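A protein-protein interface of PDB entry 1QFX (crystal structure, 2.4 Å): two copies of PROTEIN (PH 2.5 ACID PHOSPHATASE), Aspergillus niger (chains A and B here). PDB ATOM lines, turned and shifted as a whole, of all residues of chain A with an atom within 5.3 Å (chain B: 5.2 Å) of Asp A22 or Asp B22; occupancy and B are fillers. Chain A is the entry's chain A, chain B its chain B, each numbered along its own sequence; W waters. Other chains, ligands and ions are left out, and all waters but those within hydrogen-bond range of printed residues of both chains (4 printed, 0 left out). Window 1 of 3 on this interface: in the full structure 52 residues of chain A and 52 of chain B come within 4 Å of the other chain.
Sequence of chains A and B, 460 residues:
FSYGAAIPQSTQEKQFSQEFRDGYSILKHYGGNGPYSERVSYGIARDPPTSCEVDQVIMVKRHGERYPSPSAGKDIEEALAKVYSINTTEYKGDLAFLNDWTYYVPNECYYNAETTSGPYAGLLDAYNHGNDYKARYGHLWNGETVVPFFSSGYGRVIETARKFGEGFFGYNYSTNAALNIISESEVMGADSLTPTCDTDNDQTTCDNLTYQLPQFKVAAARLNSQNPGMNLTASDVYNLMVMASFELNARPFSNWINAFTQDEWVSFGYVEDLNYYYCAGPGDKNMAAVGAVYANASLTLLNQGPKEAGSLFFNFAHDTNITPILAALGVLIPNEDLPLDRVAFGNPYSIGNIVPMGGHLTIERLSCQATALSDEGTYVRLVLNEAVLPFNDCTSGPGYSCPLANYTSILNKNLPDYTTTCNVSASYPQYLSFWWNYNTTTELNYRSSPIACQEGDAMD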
ATOM      1  N   GLU A  19      22.856  -2.864 -30.517  1.00  0.00           N
ATOM      2  CA  GLU A  19      21.686  -3.382 -29.817  1.00  0.00           C
ATOM      3  C   GLU A  19      21.866  -3.140 -28.312  1.00  0.00           C
ATOM      4  O   GLU A  19      22.935  -3.410 -27.769  1.00  0.00           O
ATOM      5  CB  GLU A  19      21.563  -4.875 -30.081  1.00  0.00           C
ATOM      6  CG  GLU A  19      21.552  -5.269 -31.561  1.00  0.00           C
ATOM      7  CD  GLU A  19      21.045  -6.705 -31.769  1.00  0.00           C
ATOM      8  OE1 GLU A  19      21.248  -7.550 -30.861  1.00  0.00           O
ATOM      9  OE2 GLU A  19      20.425  -7.002 -32.826  1.00  0.00           O
ATOM     10  N   PHE A  20      20.849  -2.590 -27.650  1.00  0.00           N
ATOM     11  CA  PHE A  20      20.900  -2.305 -26.220  1.00  0.00           C
ATOM     12  C   PHE A  20      19.671  -2.919 -25.589  1.00  0.00           C
ATOM     13  O   PHE A  20      18.610  -2.297 -25.492  1.00  0.00           O
ATOM     14  CB  PHE A  20      20.971  -0.796 -25.983  1.00  0.00           C
ATOM     15  CG  PHE A  20      22.336  -0.237 -26.227  1.00  0.00           C
ATOM     16  CD1 PHE A  20      22.842  -0.145 -27.525  1.00  0.00           C
ATOM     17  CD2 PHE A  20      23.183   0.040 -25.162  1.00  0.00           C
ATOM     18  CE1 PHE A  20      24.163   0.194 -27.752  1.00  0.00           C
ATOM     19  CE2 PHE A  20      24.510   0.380 -25.383  1.00  0.00           C
ATOM     20  CZ  PHE A  20      25.001   0.451 -26.679  1.00  0.00           C
ATOM     21  N   ARG A  21      19.849  -4.154 -25.140  1.00  0.00           N
ATOM     22  CA  ARG A  21      18.797  -4.973 -24.562  1.00  0.00           C
ATOM     23  C   ARG A  21      18.786  -5.223 -23.051  1.00  0.00           C
ATOM     24  O   ARG A  21      17.855  -5.842 -22.556  1.00  0.00           O
ATOM     25  CB  ARG A  21      18.787  -6.313 -25.299  1.00  0.00           C
ATOM     26  CG  ARG A  21      18.733  -6.173 -26.828  1.00  0.00           C
ATOM     27  CD  ARG A  21      17.370  -5.618 -27.263  1.00  0.00           C
ATOM     28  NE  ARG A  21      17.269  -5.268 -28.680  1.00  0.00           N
ATOM     29  CZ  ARG A  21      16.131  -4.878 -29.273  1.00  0.00           C
ATOM     30  NH1 ARG A  21      14.983  -4.822 -28.597  1.00  0.00           N
ATOM     31  NH2 ARG A  21      16.123  -4.554 -30.556  1.00  0.00           N
ATOM     32  N   ASP A  22      19.762  -4.715 -22.306  1.00  0.00           N
ATOM     33  CA  ASP A  22      19.778  -4.926 -20.855  1.00  0.00           C
ATOM     34  C   ASP A  22      18.481  -4.581 -20.126  1.00  0.00           C
ATOM     35  O   ASP A  22      18.083  -5.270 -19.172  1.00  0.00           O
ATOM     36  CB  ASP A  22      20.906  -4.127 -20.188  1.00  0.00           C
ATOM     37  CG  ASP A  22      22.265  -4.792 -20.306  1.00  0.00           C
ATOM     38  OD1 ASP A  22      22.379  -5.949 -20.756  1.00  0.00           O
ATOM     39  OD2 ASP A  22      23.253  -4.143 -19.935  1.00  0.00           O
ATOM     40  N   GLY A  23      17.856  -3.488 -20.551  1.00  0.00           N
ATOM     41  CA  GLY A  23      16.639  -3.018 -19.914  1.00  0.00           C
ATOM     42  C   GLY A  23      15.463  -3.976 -19.925  1.00  0.00           C
ATOM     43  O   GLY A  23      14.554  -3.867 -19.095  1.00  0.00           O
ATOM     44  N   TYR A  24      15.473  -4.916 -20.860  1.00  0.00           N
ATOM     45  CA  TYR A  24      14.408  -5.877 -20.973  1.00  0.00           C
ATOM     46  C   TYR A  24      14.566  -7.065 -20.014  1.00  0.00           C
ATOM     47  O   TYR A  24      13.613  -7.852 -19.841  1.00  0.00           O
ATOM     48  CB  TYR A  24      14.355  -6.417 -22.409  1.00  0.00           C
ATOM     49  CG  TYR A  24      13.932  -5.401 -23.455  1.00  0.00           C
ATOM     50  CD1 TYR A  24      12.602  -5.022 -23.580  1.00  0.00           C
ATOM     51  CD2 TYR A  24      14.861  -4.837 -24.349  1.00  0.00           C
ATOM     52  CE1 TYR A  24      12.196  -4.118 -24.554  1.00  0.00           C
ATOM     53  CE2 TYR A  24      14.455  -3.928 -25.339  1.00  0.00           C
ATOM     54  CZ  TYR A  24      13.120  -3.575 -25.426  1.00  0.00           C
ATOM     55  OH  TYR A  24      12.676  -2.659 -26.350  1.00  0.00           O
ATOM     56  N   SER A  25      15.760  -7.238 -19.437  1.00  0.00           N
ATOM     57  CA  SER A  25      16.018  -8.364 -18.543  1.00  0.00           C
ATOM     58  C   SER A  25      15.048  -8.460 -17.359  1.00  0.00           C
ATOM     59  O   SER A  25      14.876  -7.500 -16.607  1.00  0.00           O
ATOM     60  CB  SER A  25      17.455  -8.321 -18.029  1.00  0.00           C
ATOM     61  OG  SER A  25      17.706  -9.417 -17.160  1.00  0.00           O
ATOM     62  N   LYS A  28      15.831  -7.346 -13.852  1.00  0.00           N
ATOM     63  CA  LYS A  28      15.671  -5.961 -13.428  1.00  0.00           C
ATOM     64  C   LYS A  28      14.199  -5.607 -13.225  1.00  0.00           C
ATOM     65  O   LYS A  28      13.850  -4.425 -13.101  1.00  0.00           O
ATOM     66  CB  LYS A  28      16.262  -5.017 -14.478  1.00  0.00           C
ATOM     67  CG  LYS A  28      17.751  -5.190 -14.735  1.00  0.00           C
ATOM     68  CD  LYS A  28      18.539  -5.041 -13.455  1.00  0.00           C
ATOM     69  CE  LYS A  28      20.028  -5.095 -13.735  1.00  0.00           C
ATOM     70  NZ  LYS A  28      20.798  -4.837 -12.490  1.00  0.00           N
ATOM     71  N   GLU B  19      25.331 -10.223 -15.963  1.00  0.00           N
ATOM     72  CA  GLU B  19      26.235  -9.139 -16.311  1.00  0.00           C
ATOM     73  C   GLU B  19      25.447  -8.064 -17.015  1.00  0.00           C
ATOM     74  O   GLU B  19      24.612  -8.368 -17.851  1.00  0.00           O
ATOM     75  CB  GLU B  19      27.335  -9.662 -17.233  1.00  0.00           C
ATOM     76  CG  GLU B  19      28.116 -10.868 -16.690  1.00  0.00           C
ATOM     77  CD  GLU B  19      29.406 -11.136 -17.486  1.00  0.00           C
ATOM     78  OE1 GLU B  19      29.421 -10.817 -18.695  1.00  0.00           O
ATOM     79  OE2 GLU B  19      30.411 -11.646 -16.910  1.00  0.00           O
ATOM     80  N   PHE B  20      25.668  -6.812 -16.632  1.00  0.00           N
ATOM     81  CA  PHE B  20      24.984  -5.667 -17.229  1.00  0.00           C
ATOM     82  C   PHE B  20      26.011  -4.633 -17.650  1.00  0.00           C
ATOM     83  O   PHE B  20      26.361  -3.719 -16.904  1.00  0.00           O
ATOM     84  CB  PHE B  20      23.915  -5.099 -16.277  1.00  0.00           C
ATOM     85  CG  PHE B  20      22.687  -5.954 -16.224  1.00  0.00           C
ATOM     86  CD1 PHE B  20      22.736  -7.225 -15.635  1.00  0.00           C
ATOM     87  CD2 PHE B  20      21.530  -5.571 -16.892  1.00  0.00           C
ATOM     88  CE1 PHE B  20      21.671  -8.106 -15.718  1.00  0.00           C
ATOM     89  CE2 PHE B  20      20.443  -6.447 -16.986  1.00  0.00           C
ATOM     90  CZ  PHE B  20      20.514  -7.717 -16.401  1.00  0.00           C
ATOM     91  N   ARG B  21      26.449  -4.788 -18.893  1.00  0.00           N
ATOM     92  CA  ARG B  21      27.475  -3.973 -19.487  1.00  0.00           C
ATOM     93  C   ARG B  21      27.103  -2.861 -20.496  1.00  0.00           C
ATOM     94  O   ARG B  21      27.967  -2.047 -20.847  1.00  0.00           O
ATOM     95  CB  ARG B  21      28.500  -4.931 -20.088  1.00  0.00           C
ATOM     96  CG  ARG B  21      29.027  -5.973 -19.076  1.00  0.00           C
ATOM     97  CD  ARG B  21      29.836  -5.287 -17.948  1.00  0.00           C
ATOM     98  NE  ARG B  21      30.199  -6.176 -16.841  1.00  0.00           N
ATOM     99  CZ  ARG B  21      31.012  -5.840 -15.825  1.00  0.00           C
ATOM    100  NH1 ARG B  21      31.584  -4.639 -15.761  1.00  0.00           N
ATOM    101  NH2 ARG B  21      31.266  -6.711 -14.859  1.00  0.00           N
ATOM    102  N   ASP B  22      25.839  -2.769 -20.919  1.00  0.00           N
ATOM    103  CA  ASP B  22      25.426  -1.730 -21.876  1.00  0.00           C
ATOM    104  C   ASP B  22      25.907  -0.304 -21.552  1.00  0.00           C
ATOM    105  O   ASP B  22      26.293   0.450 -22.462  1.00  0.00           O
ATOM    106  CB  ASP B  22      23.897  -1.700 -22.035  1.00  0.00           C
ATOM    107  CG  ASP B  22      23.378  -2.804 -22.933  1.00  0.00           C
ATOM    108  OD1 ASP B  22      24.182  -3.470 -23.603  1.00  0.00           O
ATOM    109  OD2 ASP B  22      22.151  -3.026 -23.002  1.00  0.00           O
ATOM    110  N   GLY B  23      25.902   0.045 -20.262  1.00  0.00           N
ATOM    111  CA  GLY B  23      26.277   1.380 -19.809  1.00  0.00           C
ATOM    112  C   GLY B  23      27.694   1.819 -20.113  1.00  0.00           C
ATOM    113  O   GLY B  23      27.997   3.026 -20.137  1.00  0.00           O
ATOM    114  N   TYR B  24      28.562   0.840 -20.326  1.00  0.00           N
ATOM    115  CA  TYR B  24      29.956   1.091 -20.637  1.00  0.00           C
ATOM    116  C   TYR B  24      30.206   1.380 -22.109  1.00  0.00           C
ATOM    117  O   TYR B  24      31.259   1.916 -22.449  1.00  0.00           O
ATOM    118  CB  TYR B  24      30.821  -0.119 -20.232  1.00  0.00           C
ATOM    119  CG  TYR B  24      30.904  -0.342 -18.742  1.00  0.00           C
ATOM    120  CD1 TYR B  24      31.685   0.489 -17.938  1.00  0.00           C
ATOM    121  CD2 TYR B  24      30.201  -1.388 -18.130  1.00  0.00           C
ATOM    122  CE1 TYR B  24      31.773   0.288 -16.556  1.00  0.00           C
ATOM    123  CE2 TYR B  24      30.281  -1.597 -16.755  1.00  0.00           C
ATOM    124  CZ  TYR B  24      31.072  -0.756 -15.971  1.00  0.00           C
ATOM    125  OH  TYR B  24      31.168  -0.966 -14.610  1.00  0.00           O
ATOM    126  N   SER B  25      29.270   1.021 -22.981  1.00  0.00           N
ATOM    127  CA  SER B  25      29.458   1.229 -24.417  1.00  0.00           C
ATOM    128  C   SER B  25      29.769   2.660 -24.798  1.00  0.00           C
ATOM    129  O   SER B  25      29.055   3.581 -24.395  1.00  0.00           O
ATOM    130  CB  SER B  25      28.242   0.775 -25.188  1.00  0.00           C
ATOM    131  OG  SER B  25      28.465   0.974 -26.558  1.00  0.00           O
ATOM    132  N   LYS B  28      27.327   5.187 -26.229  1.00  0.00           N
ATOM    133  CA  LYS B  28      26.460   5.987 -25.365  1.00  0.00           C
ATOM    134  C   LYS B  28      27.222   7.129 -24.702  1.00  0.00           C
ATOM    135  O   LYS B  28      26.703   7.768 -23.790  1.00  0.00           O
ATOM    136  CB  LYS B  28      25.826   5.099 -24.288  1.00  0.00           C
ATOM    137  CG  LYS B  28      24.973   3.970 -24.830  1.00  0.00           C
ATOM    138  CD  LYS B  28      23.805   4.505 -25.649  1.00  0.00           C
ATOM    139  CE  LYS B  28      22.835   3.407 -26.017  1.00  0.00           C
ATOM    140  NZ  LYS B  28      21.747   3.953 -26.833  1.00  0.00           N
HETATM  141  O   HOH W   1      22.209  -8.580 -19.203  1.00  0.00           O
HETATM  142  O   HOH W   2      25.449  -2.751 -26.446  1.00  0.00           O
HETATM  143  O   HOH W   3      25.200  -6.373 -20.652  1.00  0.00           O
HETATM  144  O   HOH W   4      22.368  -5.180 -24.687  1.00  0.00           O
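Water W3 lies within hydrogen-bond range of N of Arg B21 (2.7 Å), OD1 of Asp A22 (2.9 Å) and O of Glu B19 (3.5 Å). Water W4 lies within hydrogen-bond range of the side-chain carboxylate (OD1) of Asp B22 (2.7 Å) and the backbone NH (N) of Arg A21 (2.8 Å). Water W1 lies within hydrogen-bond range of the backbone carbonyl oxygen (O) of Glu B19 and the side-chain carboxylate (OD1) of Asp A22. Water W2 lies within hydrogen-bond range of the backbone carbonyl oxygen of Glu A19 (2.9 Å) and the side-chain carboxylate of Asp B22 (3.2 Å).
Of the 8 printed residues of chain B, 5 touch a printed residue of chain A. Printed residues of chain A that touch a printed residue of chain B: Phe A20, Arg A21, Asp A22, Ser A25 and Lys A28. Among the printed residues, 9 pairs touch across the chains. Among the printed residues, no Asp or Glu carboxylate lies within 4 Å of a Lys or Arg side-chain nitrogen of the other chain.
N of Arg A21 lies within hydrogen-bond range of OD2 of Asp B22, at 3.3 Å. The side-chain carboxylate (OD2) of Asp A22 lies within hydrogen-bond range of the backbone NH (N) of Arg B21. OD2 of Asp B22 lies within hydrogen-bond range of N of Asp A22.
Phe A20 touches Asp B22, and with the chains exchanged Asp A22 touches Phe B20. Phe A20 touches Ser B25, and with the chains exchanged Ser A25 touches Phe B20. Arg A21 touches Asp B22, and with the chains exchanged Asp A22 touches Arg B21. Asp A22 touches its own counterpart, Asp B22. Positions printed for both chains: 19, 20, 21, 22, 23, 24, 25 and 28. Of the 9 pairs that touch across the chains among the printed residues, 9 have their exchanged pair printed and touching as well.
Of the printed residues of chain B, Arg A21 touches Asp B22. Of the printed residues of chain B, Asp A22 touches Phe B20, Arg B21 and Asp B22. Printed residues of chain A within 4 Å of Arg B21: Asp A22. Of chain A, only Phe A20 (3.4 Å), Arg A21 (3.3 Å) and Asp A22 (3.0 Å) come within 4 Å of Asp B22. Of the printed residues of chain A, Lys B28 touches Phe A20.
Among the printed residues, merely in contact across the chains: Phe A20 with Asp B22, Phe A20 with Ser B25, Phe A20 with Lys B28, Asp A22 with Phe B20, Ser A25 with Phe B20 and Lys A28 with Phe B20.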
